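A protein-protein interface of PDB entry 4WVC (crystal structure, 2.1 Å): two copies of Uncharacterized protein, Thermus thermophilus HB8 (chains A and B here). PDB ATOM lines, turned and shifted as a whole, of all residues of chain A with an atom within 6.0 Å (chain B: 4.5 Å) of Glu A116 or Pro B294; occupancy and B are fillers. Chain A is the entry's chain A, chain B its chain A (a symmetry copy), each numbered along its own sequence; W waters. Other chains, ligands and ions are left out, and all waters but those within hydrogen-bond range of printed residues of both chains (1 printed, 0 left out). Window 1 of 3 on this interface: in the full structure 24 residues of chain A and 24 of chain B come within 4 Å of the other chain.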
ATOM      1  N   VAL A 111       0.213   0.928  22.038  1.00  0.00           N
ATOM      2  CA  VAL A 111       0.808   1.502  20.825  1.00  0.00           C
ATOM      3  C   VAL A 111       2.333   1.295  20.802  1.00  0.00           C
ATOM      4  O   VAL A 111       2.893   0.995  19.753  1.00  0.00           O
ATOM      5  CB  VAL A 111       0.389   2.976  20.627  1.00  0.00           C
ATOM      6  CG1 VAL A 111       1.167   3.648  19.493  1.00  0.00           C
ATOM      7  CG2 VAL A 111      -1.101   3.055  20.330  1.00  0.00           C
ATOM      8  N   ARG A 112       3.006   1.400  21.951  1.00  0.00           N
ATOM      9  CA  ARG A 112       4.459   1.175  21.974  1.00  0.00           C
ATOM     10  C   ARG A 112       4.819  -0.253  21.588  1.00  0.00           C
ATOM     11  O   ARG A 112       5.751  -0.479  20.824  1.00  0.00           O
ATOM     12  CB  ARG A 112       5.079   1.498  23.337  1.00  0.00           C
ATOM     13  CG  ARG A 112       6.585   1.308  23.316  1.00  0.00           C
ATOM     14  CD  ARG A 112       7.238   1.469  24.662  1.00  0.00           C
ATOM     15  NE  ARG A 112       8.660   1.165  24.552  1.00  0.00           N
ATOM     16  CZ  ARG A 112       9.552   1.259  25.538  1.00  0.00           C
ATOM     17  NH1 ARG A 112       9.195   1.658  26.761  1.00  0.00           N
ATOM     18  NH2 ARG A 112      10.817   0.955  25.287  1.00  0.00           N
ATOM     19  N   TYR A 113       4.095  -1.226  22.124  1.00  0.00           N
ATOM     20  CA  TYR A 113       4.367  -2.595  21.748  1.00  0.00           C
ATOM     21  C   TYR A 113       4.088  -2.809  20.239  1.00  0.00           C
ATOM     22  O   TYR A 113       4.915  -3.385  19.518  1.00  0.00           O
ATOM     23  CB  TYR A 113       3.559  -3.552  22.600  1.00  0.00           C
ATOM     24  CG  TYR A 113       3.736  -4.957  22.127  1.00  0.00           C
ATOM     25  CD1 TYR A 113       4.788  -5.733  22.599  1.00  0.00           C
ATOM     26  CD2 TYR A 113       2.897  -5.489  21.156  1.00  0.00           C
ATOM     27  CE1 TYR A 113       4.970  -7.013  22.156  1.00  0.00           C
ATOM     28  CE2 TYR A 113       3.094  -6.758  20.690  1.00  0.00           C
ATOM     29  CZ  TYR A 113       4.130  -7.512  21.190  1.00  0.00           C
ATOM     30  OH  TYR A 113       4.318  -8.770  20.730  1.00  0.00           O
ATOM     31  N   LEU A 114       2.943  -2.340  19.753  1.00  0.00           N
ATOM     32  CA  LEU A 114       2.641  -2.516  18.328  1.00  0.00           C
ATOM     33  C   LEU A 114       3.777  -1.946  17.460  1.00  0.00           C
ATOM     34  O   LEU A 114       4.318  -2.632  16.584  1.00  0.00           O
ATOM     35  CB  LEU A 114       1.314  -1.882  17.961  1.00  0.00           C
ATOM     36  CG  LEU A 114       0.083  -2.584  18.501  1.00  0.00           C
ATOM     37  CD1 LEU A 114      -1.195  -1.976  17.971  1.00  0.00           C
ATOM     38  CD2 LEU A 114       0.108  -4.059  18.233  1.00  0.00           C
ATOM     39  N   TYR A 115       4.162  -0.712  17.752  1.00  0.00           N
ATOM     40  CA  TYR A 115       5.254  -0.091  17.045  1.00  0.00           C
ATOM     41  C   TYR A 115       6.556  -0.917  17.065  1.00  0.00           C
ATOM     42  O   TYR A 115       7.206  -1.071  16.026  1.00  0.00           O
ATOM     43  CB  TYR A 115       5.537   1.320  17.602  1.00  0.00           C
ATOM     44  CG  TYR A 115       6.742   1.913  16.929  1.00  0.00           C
ATOM     45  CD1 TYR A 115       6.690   2.281  15.584  1.00  0.00           C
ATOM     46  CD2 TYR A 115       7.940   2.039  17.594  1.00  0.00           C
ATOM     47  CE1 TYR A 115       7.794   2.795  14.941  1.00  0.00           C
ATOM     48  CE2 TYR A 115       9.059   2.535  16.954  1.00  0.00           C
ATOM     49  CZ  TYR A 115       8.990   2.896  15.628  1.00  0.00           C
ATOM     50  OH  TYR A 115      10.095   3.390  14.996  1.00  0.00           O
ATOM     51  N   GLU A 116       6.975  -1.376  18.244  1.00  0.00           N
ATOM     52  CA  GLU A 116       8.271  -2.037  18.378  1.00  0.00           C
ATOM     53  C   GLU A 116       8.316  -3.381  17.648  1.00  0.00           C
ATOM     54  O   GLU A 116       9.347  -3.765  17.122  1.00  0.00           O
ATOM     55  CB  GLU A 116       8.643  -2.227  19.856  1.00  0.00           C
ATOM     56  CG  GLU A 116       8.939  -0.923  20.575  1.00  0.00           C
ATOM     57  CD  GLU A 116       9.847  -1.076  21.794  1.00  0.00           C
ATOM     58  OE1 GLU A 116       9.961  -2.186  22.343  1.00  0.00           O
ATOM     59  OE2 GLU A 116      10.476  -0.069  22.176  1.00  0.00           O
ATOM     60  N   LYS A 117       7.192  -4.079  17.612  1.00  0.00           N
ATOM     61  CA  LYS A 117       7.153  -5.478  17.207  1.00  0.00           C
ATOM     62  C   LYS A 117       6.523  -5.789  15.847  1.00  0.00           C
ATOM     63  O   LYS A 117       6.622  -6.909  15.395  1.00  0.00           O
ATOM     64  CB  LYS A 117       6.369  -6.264  18.258  1.00  0.00           C
ATOM     65  CG  LYS A 117       6.999  -6.316  19.642  1.00  0.00           C
ATOM     66  CD  LYS A 117       8.489  -6.619  19.620  1.00  0.00           C
ATOM     67  CE  LYS A 117       9.000  -6.937  21.018  1.00  0.00           C
ATOM     68  NZ  LYS A 117      10.473  -6.777  21.122  1.00  0.00           N
ATOM     69  N   ASP A 118       5.822  -4.842  15.242  1.00  0.00           N
ATOM     70  CA  ASP A 118       5.233  -5.067  13.919  1.00  0.00           C
ATOM     71  C   ASP A 118       6.328  -5.531  12.998  1.00  0.00           C
ATOM     72  O   ASP A 118       7.360  -4.872  12.912  1.00  0.00           O
ATOM     73  CB  ASP A 118       4.598  -3.780  13.387  1.00  0.00           C
ATOM     74  CG  ASP A 118       3.597  -4.022  12.235  1.00  0.00           C
ATOM     75  OD1 ASP A 118       3.804  -4.945  11.410  1.00  0.00           O
ATOM     76  OD2 ASP A 118       2.606  -3.249  12.140  1.00  0.00           O
ATOM     77  N   ARG A 121       7.856  -2.696   9.135  1.00  0.00           N
ATOM     78  CA  ARG A 121       8.459  -1.520   9.723  1.00  0.00           C
ATOM     79  C   ARG A 121       7.959  -0.220   9.090  1.00  0.00           C
ATOM     80  O   ARG A 121       7.833   0.781   9.791  1.00  0.00           O
ATOM     81  CB  ARG A 121       9.981  -1.610   9.672  1.00  0.00           C
ATOM     82  CG  ARG A 121      10.594  -2.859  10.314  1.00  0.00           C
ATOM     83  CD  ARG A 121      10.057  -3.169  11.715  1.00  0.00           C
ATOM     84  NE  ARG A 121      10.160  -1.999  12.594  1.00  0.00           N
ATOM     85  CZ  ARG A 121       9.340  -1.716  13.606  1.00  0.00           C
ATOM     86  NH1 ARG A 121       8.341  -2.530  13.950  1.00  0.00           N
ATOM     87  NH2 ARG A 121       9.530  -0.607  14.299  1.00  0.00           N
ATOM     88  N   ALA A 124       4.487   0.072  10.766  1.00  0.00           N
ATOM     89  CA  ALA A 124       4.776   0.492  12.136  1.00  0.00           C
ATOM     90  C   ALA A 124       4.964   2.010  12.217  1.00  0.00           C
ATOM     91  O   ALA A 124       4.282   2.680  12.984  1.00  0.00           O
ATOM     92  CB  ALA A 124       6.029  -0.217  12.642  1.00  0.00           C
ATOM     93  N   ALA A 250       9.146   6.954  25.188  1.00  0.00           N
ATOM     94  CA  ALA A 250       9.953   6.027  24.385  1.00  0.00           C
ATOM     95  C   ALA A 250       9.636   6.160  22.904  1.00  0.00           C
ATOM     96  O   ALA A 250      10.547   6.302  22.070  1.00  0.00           O
ATOM     97  CB  ALA A 250       9.737   4.588  24.824  1.00  0.00           C
ATOM     98  N   LEU A 254      12.108   7.301  19.860  1.00  0.00           N
ATOM     99  CA  LEU A 254      12.287   6.344  18.754  1.00  0.00           C
ATOM    100  C   LEU A 254      11.862   6.924  17.435  1.00  0.00           C
ATOM    101  O   LEU A 254      12.503   6.680  16.420  1.00  0.00           O
ATOM    102  CB  LEU A 254      11.481   5.054  19.008  1.00  0.00           C
ATOM    103  CG  LEU A 254      12.068   4.125  20.072  1.00  0.00           C
ATOM    104  CD1 LEU A 254      11.018   3.143  20.522  1.00  0.00           C
ATOM    105  CD2 LEU A 254      13.300   3.406  19.540  1.00  0.00           C
ATOM    106  N   SER B 286      21.027  -0.343  23.428  1.00  0.00           N
ATOM    107  CA  SER B 286      21.225   0.889  22.693  1.00  0.00           C
ATOM    108  C   SER B 286      20.122   0.966  21.640  1.00  0.00           C
ATOM    109  O   SER B 286      19.576  -0.061  21.229  1.00  0.00           O
ATOM    110  CB  SER B 286      22.626   0.945  22.058  1.00  0.00           C
ATOM    111  OG  SER B 286      23.624   0.946  23.051  1.00  0.00           O
ATOM    112  N   TRP B 287      19.825   2.176  21.196  1.00  0.00           N
ATOM    113  CA  TRP B 287      18.752   2.403  20.238  1.00  0.00           C
ATOM    114  C   TRP B 287      19.261   2.980  18.909  1.00  0.00           C
ATOM    115  O   TRP B 287      20.107   3.880  18.875  1.00  0.00           O
ATOM    116  CB  TRP B 287      17.736   3.358  20.850  1.00  0.00           C
ATOM    117  CG  TRP B 287      16.805   2.757  21.839  1.00  0.00           C
ATOM    118  CD1 TRP B 287      16.791   1.479  22.303  1.00  0.00           C
ATOM    119  CD2 TRP B 287      15.746   3.435  22.504  1.00  0.00           C
ATOM    120  NE1 TRP B 287      15.780   1.319  23.210  1.00  0.00           N
ATOM    121  CE2 TRP B 287      15.130   2.511  23.362  1.00  0.00           C
ATOM    122  CE3 TRP B 287      15.276   4.738  22.468  1.00  0.00           C
ATOM    123  CZ2 TRP B 287      14.065   2.847  24.158  1.00  0.00           C
ATOM    124  CZ3 TRP B 287      14.219   5.068  23.250  1.00  0.00           C
ATOM    125  CH2 TRP B 287      13.620   4.139  24.081  1.00  0.00           C
ATOM    126  N   GLU B 293      14.384   1.901  16.174  1.00  0.00           N
ATOM    127  CA  GLU B 293      14.194   0.656  16.923  1.00  0.00           C
ATOM    128  C   GLU B 293      15.264   0.435  17.989  1.00  0.00           C
ATOM    129  O   GLU B 293      16.436   0.811  17.820  1.00  0.00           O
ATOM    130  CB  GLU B 293      14.286  -0.556  15.998  1.00  0.00           C
ATOM    131  CG  GLU B 293      13.300  -0.609  14.850  1.00  0.00           C
ATOM    132  CD  GLU B 293      13.639  -1.734  13.891  1.00  0.00           C
ATOM    133  OE1 GLU B 293      13.543  -2.903  14.327  1.00  0.00           O
ATOM    134  OE2 GLU B 293      13.978  -1.459  12.723  1.00  0.00           O
ATOM    135  N   PRO B 294      14.887  -0.263  19.057  1.00  0.00           N
ATOM    136  CA  PRO B 294      15.931  -0.859  19.868  1.00  0.00           C
ATOM    137  C   PRO B 294      16.852  -1.825  19.078  1.00  0.00           C
ATOM    138  O   PRO B 294      16.396  -2.531  18.196  1.00  0.00           O
ATOM    139  CB  PRO B 294      15.145  -1.635  20.918  1.00  0.00           C
ATOM    140  CG  PRO B 294      13.798  -1.010  20.960  1.00  0.00           C
ATOM    141  CD  PRO B 294      13.537  -0.574  19.558  1.00  0.00           C
ATOM    142  N   ILE B 295      18.145  -1.821  19.393  1.00  0.00           N
ATOM    143  CA  ILE B 295      19.090  -2.798  18.881  1.00  0.00           C
ATOM    144  C   ILE B 295      19.147  -3.946  19.875  1.00  0.00           C
ATOM    145  O   ILE B 295      19.772  -3.847  20.944  1.00  0.00           O
ATOM    146  CB  ILE B 295      20.496  -2.190  18.749  1.00  0.00           C
ATOM    147  CG1 ILE B 295      20.478  -0.948  17.848  1.00  0.00           C
ATOM    148  CG2 ILE B 295      21.491  -3.249  18.234  1.00  0.00           C
ATOM    149  CD1 ILE B 295      21.665  -0.022  18.068  1.00  0.00           C
ATOM    150  N   ALA B 296      18.484  -5.039  19.546  1.00  0.00           N
ATOM    151  CA  ALA B 296      18.380  -6.163  20.466  1.00  0.00           C
ATOM    152  C   ALA B 296      19.680  -6.991  20.520  1.00  0.00           C
ATOM    153  O   ALA B 296      19.712  -8.129  20.082  1.00  0.00           O
ATOM    154  CB  ALA B 296      17.195  -7.044  20.093  1.00  0.00           C
HETATM  155  O   HOH W   1      11.470  -2.539  17.023  1.00  0.00           O
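Among the printed residues, merely in contact across the chains: Arg A112 with Trp B287 (3.9 Å), Glu A116 with Pro B294 (3.7 Å), Ala A250 with Trp B287 (3.98 Å), Leu A254 with Trp B287 (3.8 Å), Leu A254 with Glu B293 (3.8 Å) and Leu A254 with Pro B294 (3.99 Å).
Of the 12 printed residues of chain A, 5 touch a printed residue of chain B. Hydrophobic or aromatic side chains of chain A within 4 Å of the printed part of chain B: Ala A250 and Leu A254. Among the printed residues, 7 pairs touch across the chains. Among the printed residues, Asp or Glu carboxylates within 4 Å of a Lys or Arg side-chain nitrogen of the other chain: Arg A121 with Glu B293.
No position is printed for both chains. Of the 7 pairs that touch across the chains among the printed residues, none has its exchanged pair printed and touching as well.
Water W1 lies within hydrogen-bond range of the backbone carbonyl oxygen of Glu A116 and the side-chain carboxylate of Glu B293.
NE of Arg A121 is in salt-bridge range of OE2 of Glu B293.
The side-chain carboxylate of Glu A116 lies within salt-bridge range of the guanidinium group of Arg A112 (3.2 Å). The guanidinium group (NH1) of Arg A121 sits at hydrogen-bond distance from the backbone carbonyl oxygen (O) of Tyr A115 (2.8 Å). The guanidinium group of Arg A121 sits at hydrogen-bond distance from the backbone carbonyl oxygen of Asp A118, 2.7 Å away.
Of chain B, only Pro B294 (3.7 Å) comes within 4 Å of Glu A116. Printed residues of chain A within 4 Å of Pro B294: Glu A116 and Leu A254. Printed residues of chain B within 4 Å of Ala A250: Trp B287 (3.98 Å). Printed residues of chain B within 4 Å of Arg A112: Trp B287 (3.9 Å). Printed residues of chain A within 4 Å of Glu B293: Arg A121 and Leu A254. Ala B296 touches none of the printed residues of chain A. Lys A117 touches none of the printed residues of chain B. The nearest printed residue of chain A that does not touch Pro B294 is Arg A112 (5.6 Å).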
